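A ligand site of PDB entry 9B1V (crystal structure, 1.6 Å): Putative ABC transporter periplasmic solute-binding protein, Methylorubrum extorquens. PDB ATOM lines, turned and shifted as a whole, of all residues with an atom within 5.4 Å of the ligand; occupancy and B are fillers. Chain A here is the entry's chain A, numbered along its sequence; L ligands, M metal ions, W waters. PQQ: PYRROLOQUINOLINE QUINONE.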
ATOM      1  N   GLY A   8      -9.231   3.581  11.180  1.00  0.00           N
ATOM      2  CA  GLY A   8      -8.128   4.194  11.914  1.00  0.00           C
ATOM      3  C   GLY A   8      -7.937   5.637  11.502  1.00  0.00           C
ATOM      4  O   GLY A   8      -7.861   5.888  10.298  1.00  0.00           O
ATOM      5  N   VAL A   9      -7.878   6.534  12.484  1.00  0.00           N
ATOM      6  CA  VAL A   9      -7.789   7.989  12.189  1.00  0.00           C
ATOM      7  C   VAL A   9      -6.648   8.630  12.981  1.00  0.00           C
ATOM      8  O   VAL A   9      -6.374   8.215  14.089  1.00  0.00           O
ATOM      9  CB  VAL A   9      -9.124   8.724  12.492  1.00  0.00           C
ATOM     10  CG1 VAL A   9     -10.271   8.188  11.646  1.00  0.00           C
ATOM     11  CG2 VAL A   9      -9.475   8.700  13.965  1.00  0.00           C
ATOM     12  N   LEU A  10      -6.067   9.673  12.384  1.00  0.00           N
ATOM     13  CA  LEU A  10      -4.997  10.430  13.068  1.00  0.00           C
ATOM     14  C   LEU A  10      -5.616  11.602  13.824  1.00  0.00           C
ATOM     15  O   LEU A  10      -6.618  12.145  13.411  1.00  0.00           O
ATOM     16  CB  LEU A  10      -4.036  10.950  11.999  1.00  0.00           C
ATOM     17  CG  LEU A  10      -3.391   9.884  11.115  1.00  0.00           C
ATOM     18  CD1 LEU A  10      -2.364  10.510  10.194  1.00  0.00           C
ATOM     19  CD2 LEU A  10      -2.747   8.797  11.960  1.00  0.00           C
ATOM     20  N   PHE A  12      -4.656  14.652  14.126  1.00  0.00           N
ATOM     21  CA  PHE A  12      -4.509  15.946  13.436  1.00  0.00           C
ATOM     22  C   PHE A  12      -5.023  15.830  12.008  1.00  0.00           C
ATOM     23  O   PHE A  12      -4.843  16.740  11.229  1.00  0.00           O
ATOM     24  CB  PHE A  12      -3.047  16.366  13.432  1.00  0.00           C
ATOM     25  CG  PHE A  12      -2.070  15.317  12.963  1.00  0.00           C
ATOM     26  CD1 PHE A  12      -1.872  15.088  11.615  1.00  0.00           C
ATOM     27  CD2 PHE A  12      -1.354  14.565  13.868  1.00  0.00           C
ATOM     28  CE1 PHE A  12      -0.986  14.113  11.180  1.00  0.00           C
ATOM     29  CE2 PHE A  12      -0.472  13.591  13.441  1.00  0.00           C
ATOM     30  CZ  PHE A  12      -0.285  13.369  12.098  1.00  0.00           C
ATOM     31  N   GLY A  13      -5.658  14.698  11.730  1.00  0.00           N
ATOM     32  CA  GLY A  13      -6.184  14.474  10.380  1.00  0.00           C
ATOM     33  C   GLY A  13      -7.599  15.006  10.173  1.00  0.00           C
ATOM     34  O   GLY A  13      -8.255  15.302  11.144  1.00  0.00           O
ATOM     35  N   THR A  14      -8.029  15.018   8.910  1.00  0.00           N
ATOM     36  CA  THR A  14      -9.359  15.562   8.574  1.00  0.00           C
ATOM     37  C   THR A  14     -10.404  14.433   8.467  1.00  0.00           C
ATOM     38  O   THR A  14     -11.554  14.744   8.446  1.00  0.00           O
ATOM     39  CB  THR A  14      -9.285  16.346   7.259  1.00  0.00           C
ATOM     40  OG1 THR A  14      -9.031  15.473   6.166  1.00  0.00           O
ATOM     41  CG2 THR A  14      -8.226  17.429   7.289  1.00  0.00           C
ATOM     42  N   ALA A  15      -9.979  13.168   8.430  1.00  0.00           N
ATOM     43  CA  ALA A  15     -10.939  12.041   8.274  1.00  0.00           C
ATOM     44  C   ALA A  15     -11.898  11.999   9.457  1.00  0.00           C
ATOM     45  O   ALA A  15     -13.024  11.609   9.293  1.00  0.00           O
ATOM     46  CB  ALA A  15     -10.202  10.739   8.146  1.00  0.00           C
ATOM     47  N   SER A  16     -11.404  12.370  10.644  1.00  0.00           N
ATOM     48  CA  SER A  16     -12.260  12.403  11.853  1.00  0.00           C
ATOM     49  C   SER A  16     -13.481  13.289  11.637  1.00  0.00           C
ATOM     50  O   SER A  16     -14.467  13.113  12.346  1.00  0.00           O
ATOM     51  CB  SER A  16     -11.434  12.882  13.014  1.00  0.00           C
ATOM     52  OG  SER A  16     -10.462  11.919  13.358  1.00  0.00           O
ATOM     53  N   ASN A  43       1.085   8.229  11.755  1.00  0.00           N
ATOM     54  CA  ASN A  43       1.009   7.461  10.497  1.00  0.00           C
ATOM     55  C   ASN A  43       1.763   6.141  10.615  1.00  0.00           C
ATOM     56  O   ASN A  43       1.334   5.180  10.049  1.00  0.00           O
ATOM     57  CB  ASN A  43       1.558   8.276   9.350  1.00  0.00           C
ATOM     58  CG  ASN A  43       0.762   8.038   8.097  1.00  0.00           C
ATOM     59  OD1 ASN A  43      -0.469   7.990   8.141  1.00  0.00           O
ATOM     60  ND2 ASN A  43       1.449   7.836   6.980  1.00  0.00           N
ATOM     61  N   VAL A  59      -6.657   6.174   6.344  1.00  0.00           N
ATOM     62  CA  VAL A  59      -6.509   7.156   5.246  1.00  0.00           C
ATOM     63  C   VAL A  59      -5.023   7.204   4.910  1.00  0.00           C
ATOM     64  O   VAL A  59      -4.207   7.169   5.813  1.00  0.00           O
ATOM     65  CB  VAL A  59      -7.086   8.539   5.629  1.00  0.00           C
ATOM     66  CG1 VAL A  59      -6.803   9.577   4.553  1.00  0.00           C
ATOM     67  CG2 VAL A  59      -8.580   8.434   5.892  1.00  0.00           C
ATOM     68  N   GLY A  60      -4.718   7.221   3.618  1.00  0.00           N
ATOM     69  CA  GLY A  60      -3.325   7.298   3.222  1.00  0.00           C
ATOM     70  C   GLY A  60      -3.162   7.737   1.793  1.00  0.00           C
ATOM     71  O   GLY A  60      -4.143   8.127   1.190  1.00  0.00           O
ATOM     72  N   ASP A  61      -1.938   7.658   1.296  1.00  0.00           N
ATOM     73  CA  ASP A  61      -1.667   8.197  -0.041  1.00  0.00           C
ATOM     74  C   ASP A  61      -1.542   7.076  -1.066  1.00  0.00           C
ATOM     75  O   ASP A  61      -1.290   5.934  -0.692  1.00  0.00           O
ATOM     76  CB  ASP A  61      -0.486   9.154   0.024  1.00  0.00           C
ATOM     77  CG  ASP A  61       0.824   8.448   0.253  1.00  0.00           C
ATOM     78  OD1 ASP A  61       1.404   7.975  -0.725  1.00  0.00           O
ATOM     79  OD2 ASP A  61       1.225   8.372   1.423  1.00  0.00           O
ATOM     80  N   TYR A  80     -10.095  10.112  -1.448  1.00  0.00           N
ATOM     81  CA  TYR A  80     -10.627  10.784  -0.232  1.00  0.00           C
ATOM     82  C   TYR A  80     -10.640  12.291  -0.451  1.00  0.00           C
ATOM     83  O   TYR A  80     -11.604  12.932  -0.065  1.00  0.00           O
ATOM     84  CB  TYR A  80      -9.802  10.406   1.012  1.00  0.00           C
ATOM     85  CG  TYR A  80     -10.076  11.261   2.232  1.00  0.00           C
ATOM     86  CD1 TYR A  80     -11.166  11.005   3.050  1.00  0.00           C
ATOM     87  CD2 TYR A  80      -9.250  12.319   2.558  1.00  0.00           C
ATOM     88  CE1 TYR A  80     -11.432  11.789   4.152  1.00  0.00           C
ATOM     89  CE2 TYR A  80      -9.509  13.123   3.649  1.00  0.00           C
ATOM     90  CZ  TYR A  80     -10.593  12.852   4.461  1.00  0.00           C
ATOM     91  OH  TYR A  80     -10.848  13.645   5.533  1.00  0.00           O
ATOM     92  N   THR A  83      -7.289  17.723  -2.122  1.00  0.00           N
ATOM     93  CA  THR A  83      -6.524  18.780  -1.421  1.00  0.00           C
ATOM     94  C   THR A  83      -5.380  18.104  -0.649  1.00  0.00           C
ATOM     95  O   THR A  83      -5.646  17.242   0.171  1.00  0.00           O
ATOM     96  CB  THR A  83      -7.436  19.603  -0.503  1.00  0.00           C
ATOM     97  OG1 THR A  83      -8.415  20.241  -1.302  1.00  0.00           O
ATOM     98  CG2 THR A  83      -6.689  20.646   0.304  1.00  0.00           C
ATOM     99  N   GLU A  84      -4.151  18.462  -0.990  1.00  0.00           N
ATOM    100  CA  GLU A  84      -2.997  17.788  -0.370  1.00  0.00           C
ATOM    101  C   GLU A  84      -1.776  18.691  -0.344  1.00  0.00           C
ATOM    102  O   GLU A  84      -1.511  19.364  -1.336  1.00  0.00           O
ATOM    103  CB  GLU A  84      -2.610  16.510  -1.131  1.00  0.00           C
ATOM    104  CG  GLU A  84      -2.572  16.694  -2.645  1.00  0.00           C
ATOM    105  CD  GLU A  84      -3.580  15.919  -3.476  1.00  0.00           C
ATOM    106  OE1 GLU A  84      -4.313  15.091  -2.920  1.00  0.00           O
ATOM    107  OE2 GLU A  84      -3.638  16.181  -4.690  1.00  0.00           O
ATOM    108  N   GLY A  85      -1.090  18.706   0.791  1.00  0.00           N
ATOM    109  CA  GLY A  85       0.201  19.396   0.863  1.00  0.00           C
ATOM    110  C   GLY A  85       0.190  20.887   1.030  1.00  0.00           C
ATOM    111  O   GLY A  85      -0.649  21.554   0.439  1.00  0.00           O
ATOM    112  N   ASP A 114       7.596  10.438   1.607  1.00  0.00           N
ATOM    113  CA  ASP A 114       6.270  11.098   1.624  1.00  0.00           C
ATOM    114  C   ASP A 114       5.878  11.553   0.217  1.00  0.00           C
ATOM    115  O   ASP A 114       6.708  12.128  -0.475  1.00  0.00           O
ATOM    116  CB  ASP A 114       6.185  12.285   2.590  1.00  0.00           C
ATOM    117  CG  ASP A 114       4.821  12.942   2.623  1.00  0.00           C
ATOM    118  OD1 ASP A 114       3.940  12.454   3.344  1.00  0.00           O
ATOM    119  OD2 ASP A 114       4.643  13.942   1.915  1.00  0.00           O
ATOM    120  N   LYS A 115       4.618  11.359  -0.111  1.00  0.00           N
ATOM    121  CA  LYS A 115       4.131  11.700  -1.466  1.00  0.00           C
ATOM    122  C   LYS A 115       4.348  13.176  -1.793  1.00  0.00           C
ATOM    123  O   LYS A 115       4.636  13.465  -2.924  1.00  0.00           O
ATOM    124  CB  LYS A 115       2.665  11.292  -1.623  1.00  0.00           C
ATOM    125  CG  LYS A 115       1.624  12.192  -0.969  1.00  0.00           C
ATOM    126  CD  LYS A 115       1.604  12.150   0.542  1.00  0.00           C
ATOM    127  CE  LYS A 115       0.480  12.955   1.137  1.00  0.00           C
ATOM    128  NZ  LYS A 115       0.637  13.130   2.598  1.00  0.00           N
ATOM    129  N   ASN A 116       4.140  14.048  -0.823  1.00  0.00           N
ATOM    130  CA  ASN A 116       4.257  15.495  -1.104  1.00  0.00           C
ATOM    131  C   ASN A 116       5.735  15.823  -1.377  1.00  0.00           C
ATOM    132  O   ASN A 116       6.001  16.685  -2.197  1.00  0.00           O
ATOM    133  CB  ASN A 116       3.704  16.366   0.036  1.00  0.00           C
ATOM    134  CG  ASN A 116       2.219  16.207   0.222  1.00  0.00           C
ATOM    135  OD1 ASN A 116       1.487  15.986  -0.733  1.00  0.00           O
ATOM    136  ND2 ASN A 116       1.758  16.315   1.464  1.00  0.00           N
ATOM    137  N   LEU A 160       4.037  20.438   4.850  1.00  0.00           N
ATOM    138  CA  LEU A 160       3.131  19.812   5.840  1.00  0.00           C
ATOM    139  C   LEU A 160       1.846  19.337   5.164  1.00  0.00           C
ATOM    140  O   LEU A 160       1.693  19.547   3.979  1.00  0.00           O
ATOM    141  CB  LEU A 160       2.766  20.890   6.857  1.00  0.00           C
ATOM    142  CG  LEU A 160       3.936  21.545   7.594  1.00  0.00           C
ATOM    143  CD1 LEU A 160       3.474  22.786   8.347  1.00  0.00           C
ATOM    144  CD2 LEU A 160       4.579  20.560   8.558  1.00  0.00           C
ATOM    145  N   TYR A 161       1.001  18.701   5.948  1.00  0.00           N
ATOM    146  CA  TYR A 161      -0.333  18.343   5.421  1.00  0.00           C
ATOM    147  C   TYR A 161      -1.096  19.650   5.256  1.00  0.00           C
ATOM    148  O   TYR A 161      -0.894  20.596   6.007  1.00  0.00           O
ATOM    149  CB  TYR A 161      -1.036  17.354   6.354  1.00  0.00           C
ATOM    150  CG  TYR A 161      -0.460  15.957   6.455  1.00  0.00           C
ATOM    151  CD1 TYR A 161       0.691  15.593   5.778  1.00  0.00           C
ATOM    152  CD2 TYR A 161      -1.080  14.984   7.246  1.00  0.00           C
ATOM    153  CE1 TYR A 161       1.221  14.318   5.871  1.00  0.00           C
ATOM    154  CE2 TYR A 161      -0.560  13.702   7.346  1.00  0.00           C
ATOM    155  CZ  TYR A 161       0.592  13.374   6.664  1.00  0.00           C
ATOM    156  OH  TYR A 161       1.107  12.109   6.748  1.00  0.00           O
ATOM    157  N   TRP A 162      -1.993  19.672   4.293  1.00  0.00           N
ATOM    158  CA  TRP A 162      -2.688  20.928   3.934  1.00  0.00           C
ATOM    159  C   TRP A 162      -3.372  21.600   5.133  1.00  0.00           C
ATOM    160  O   TRP A 162      -3.393  22.833   5.157  1.00  0.00           O
ATOM    161  CB  TRP A 162      -3.678  20.602   2.815  1.00  0.00           C
ATOM    162  CG  TRP A 162      -4.982  19.972   3.243  1.00  0.00           C
ATOM    163  CD1 TRP A 162      -5.322  18.651   3.138  1.00  0.00           C
ATOM    164  CD2 TRP A 162      -6.145  20.645   3.774  1.00  0.00           C
ATOM    165  NE1 TRP A 162      -6.586  18.451   3.605  1.00  0.00           N
ATOM    166  CE2 TRP A 162      -7.116  19.652   3.996  1.00  0.00           C
ATOM    167  CE3 TRP A 162      -6.442  21.971   4.099  1.00  0.00           C
ATOM    168  CZ2 TRP A 162      -8.367  19.954   4.522  1.00  0.00           C
ATOM    169  CZ3 TRP A 162      -7.674  22.262   4.626  1.00  0.00           C
ATOM    170  CH2 TRP A 162      -8.627  21.274   4.821  1.00  0.00           C
ATOM    171  N   GLN A 163      -3.913  20.843   6.061  1.00  0.00           N
ATOM    172  CA  GLN A 163      -4.715  21.458   7.168  1.00  0.00           C
ATOM    173  C   GLN A 163      -3.856  22.296   8.118  1.00  0.00           C
ATOM    174  O   GLN A 163      -4.408  23.087   8.868  1.00  0.00           O
ATOM    175  CB  GLN A 163      -5.504  20.380   7.917  1.00  0.00           C
ATOM    176  CG  GLN A 163      -4.647  19.336   8.612  1.00  0.00           C
ATOM    177  CD  GLN A 163      -4.427  18.111   7.762  1.00  0.00           C
ATOM    178  OE1 GLN A 163      -4.398  18.181   6.542  1.00  0.00           O
ATOM    179  NE2 GLN A 163      -4.280  16.974   8.410  1.00  0.00           N
ATOM    180  N   ILE A 195      -4.756  11.414  -1.883  1.00  0.00           N
ATOM    181  CA  ILE A 195      -5.155  10.929  -0.539  1.00  0.00           C
ATOM    182  C   ILE A 195      -6.409  10.078  -0.723  1.00  0.00           C
ATOM    183  O   ILE A 195      -7.306  10.470  -1.465  1.00  0.00           O
ATOM    184  CB  ILE A 195      -5.416  12.077   0.450  1.00  0.00           C
ATOM    185  CG1 ILE A 195      -4.340  13.163   0.387  1.00  0.00           C
ATOM    186  CG2 ILE A 195      -5.557  11.544   1.871  1.00  0.00           C
ATOM    187  CD1 ILE A 195      -2.955  12.649   0.689  1.00  0.00           C
HETATM  188  N1  PQQ L   1      -5.397  12.269   7.080  1.00  0.00           N
HETATM  189  C2  PQQ L   1      -5.477  11.085   7.784  1.00  0.00           C
HETATM  190  C2X PQQ L   1      -6.491  10.842   8.782  1.00  0.00           C
HETATM  191  O2A PQQ L   1      -7.255  11.745   9.019  1.00  0.00           O
HETATM  192  O2B PQQ L   1      -6.480   9.784   9.364  1.00  0.00           O
HETATM  193  C3  PQQ L   1      -4.438  10.284   7.382  1.00  0.00           C
HETATM  194  C3A PQQ L   1      -3.698  10.973   6.404  1.00  0.00           C
HETATM  195  C1A PQQ L   1      -4.343  12.189   6.209  1.00  0.00           C
HETATM  196  C4  PQQ L   1      -2.516  10.602   5.642  1.00  0.00           C
HETATM  197  O4  PQQ L   1      -1.966   9.533   5.688  1.00  0.00           O
HETATM  198  C5  PQQ L   1      -1.934  11.685   4.725  1.00  0.00           C
HETATM  199  O5  PQQ L   1      -0.966  11.409   4.047  1.00  0.00           O
HETATM  200  C6A PQQ L   1      -2.606  12.985   4.650  1.00  0.00           C
HETATM  201  N6  PQQ L   1      -2.048  13.889   3.863  1.00  0.00           N
HETATM  202  C7  PQQ L   1      -2.609  15.070   3.737  1.00  0.00           C
HETATM  203  C7X PQQ L   1      -1.882  16.047   2.862  1.00  0.00           C
HETATM  204  O7A PQQ L   1      -2.302  17.201   2.831  1.00  0.00           O
HETATM  205  O7B PQQ L   1      -0.878  15.631   2.280  1.00  0.00           O
HETATM  206  C8  PQQ L   1      -3.798  15.423   4.397  1.00  0.00           C
HETATM  207  C9  PQQ L   1      -4.422  14.495   5.223  1.00  0.00           C
HETATM  208  C9X PQQ L   1      -5.711  14.897   5.883  1.00  0.00           C
HETATM  209  O9A PQQ L   1      -5.831  14.825   7.094  1.00  0.00           O
HETATM  210  O9B PQQ L   1      -6.609  15.280   5.131  1.00  0.00           O
HETATM  211  C9A PQQ L   1      -3.820  13.208   5.341  1.00  0.00           C
HETATM  212 GD    GD M   1      -0.502   6.322   4.818  1.00  0.00          GD
HETATM  213  O   HOH W   1      -5.881   7.193   9.030  1.00  0.00           O
HETATM  214  O   HOH W   2       0.276   9.044   3.594  1.00  0.00           O
HETATM  215  O   HOH W   3      -8.441  12.039  11.406  1.00  0.00           O
HETATM  216  O   HOH W   4      -7.072  15.727   2.379  1.00  0.00           O
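An oxygen (O9A) of the ligand lies within hydrogen-bond range of the backbone NH of Thr 14 (2.9 Å). The side-chain hydroxyl (OG1) of Thr 14 lies within hydrogen-bond range of an oxygen (O9B) of the ligand, 2.6 Å away. The side-chain amino group (NZ) of Lys 115 is in salt-bridge range of an oxygen (O7B) of the ligand (2.9 Å). The backbone NH (N) of Gly 85 lies within hydrogen-bond range of an oxygen (O7A) of the ligand (2.8 Å). An oxygen (O7B) of the ligand is in hydrogen-bond range of the side-chain amide nitrogen (ND2) of Asn 116, 2.8 Å away. The backbone NH (N) of Trp 162 sits at hydrogen-bond distance from an oxygen (O7A) of the ligand (2.9 Å). An oxygen (O9A) of the ligand is in hydrogen-bond range of the side-chain amide nitrogen of Gln 163, at 3.0 Å. An oxygen (O2B) of the ligand is in hydrogen-bond range of the backbone NH (N) of Leu 10 (3.1 Å). O2A of the ligand sits at hydrogen-bond distance from N of Ala 15 (3.1 Å). The side-chain amide oxygen (OD1) of Asn 43 lies close to an oxygen (O4) of the ligand, at 3.3 Å. An oxygen (O5) of the ligand is in hydrogen-bond range of the side-chain hydroxyl (OH) of Tyr 161, 3.5 Å away.
The side-chain hydroxyl of Tyr 80 sits at hydrogen-bond distance from the side-chain hydroxyl of Thr 14 (2.7 Å). The side-chain carboxylate (OD1) of Asp 114 is in salt-bridge range of the side-chain amino group (NZ) of Lys 115 (3.5 Å). The backbone NH (N) of Asn 116 lies within hydrogen-bond range of the side-chain carboxylate (OD2) of Asp 114 (2.8 Å). The backbone carbonyl oxygen (O) of Phe 12 is in hydrogen-bond range of the side-chain amide nitrogen (NE2) of Gln 163 (2.9 Å). The backbone NH of Ala 15 is in hydrogen-bond range of the side-chain hydroxyl of Tyr 80, at 3.1 Å. O of Ile 195 sits at hydrogen-bond distance from N of Tyr 80, at 2.8 Å.
An oxygen (O4) of the ligand lies close to the backbone carbonyl oxygen (O) of Val 59 (3.3 Å). Merely in contact with the ligand: Val 9, Gly 13, Gly 60, Tyr 80, Glu 84 and Ile 195. Hydrophobic or aromatic side chains that line the ligand: Leu 10, Ala 15, Val 59, Tyr 80, Tyr 161, Trp 162 and Ile 195. Of the 24 residues printed, 17 come within 4 Å of the ligand.
Water W1 lies within hydrogen-bond range of O2B of the ligand, O of Gly 8 and N of Val 59. Water W3 lies within hydrogen-bond range of O2A of the ligand, O of Leu 10, OG of Ser 16 and O of Gly 13. Water W2 bridges OD2 of Asp 61 (2.5 Å) and O5 of the ligand (2.7 Å). Water W4 lies within hydrogen-bond range of O9B of the ligand, NE1 of Trp 162 and O of Thr 83.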
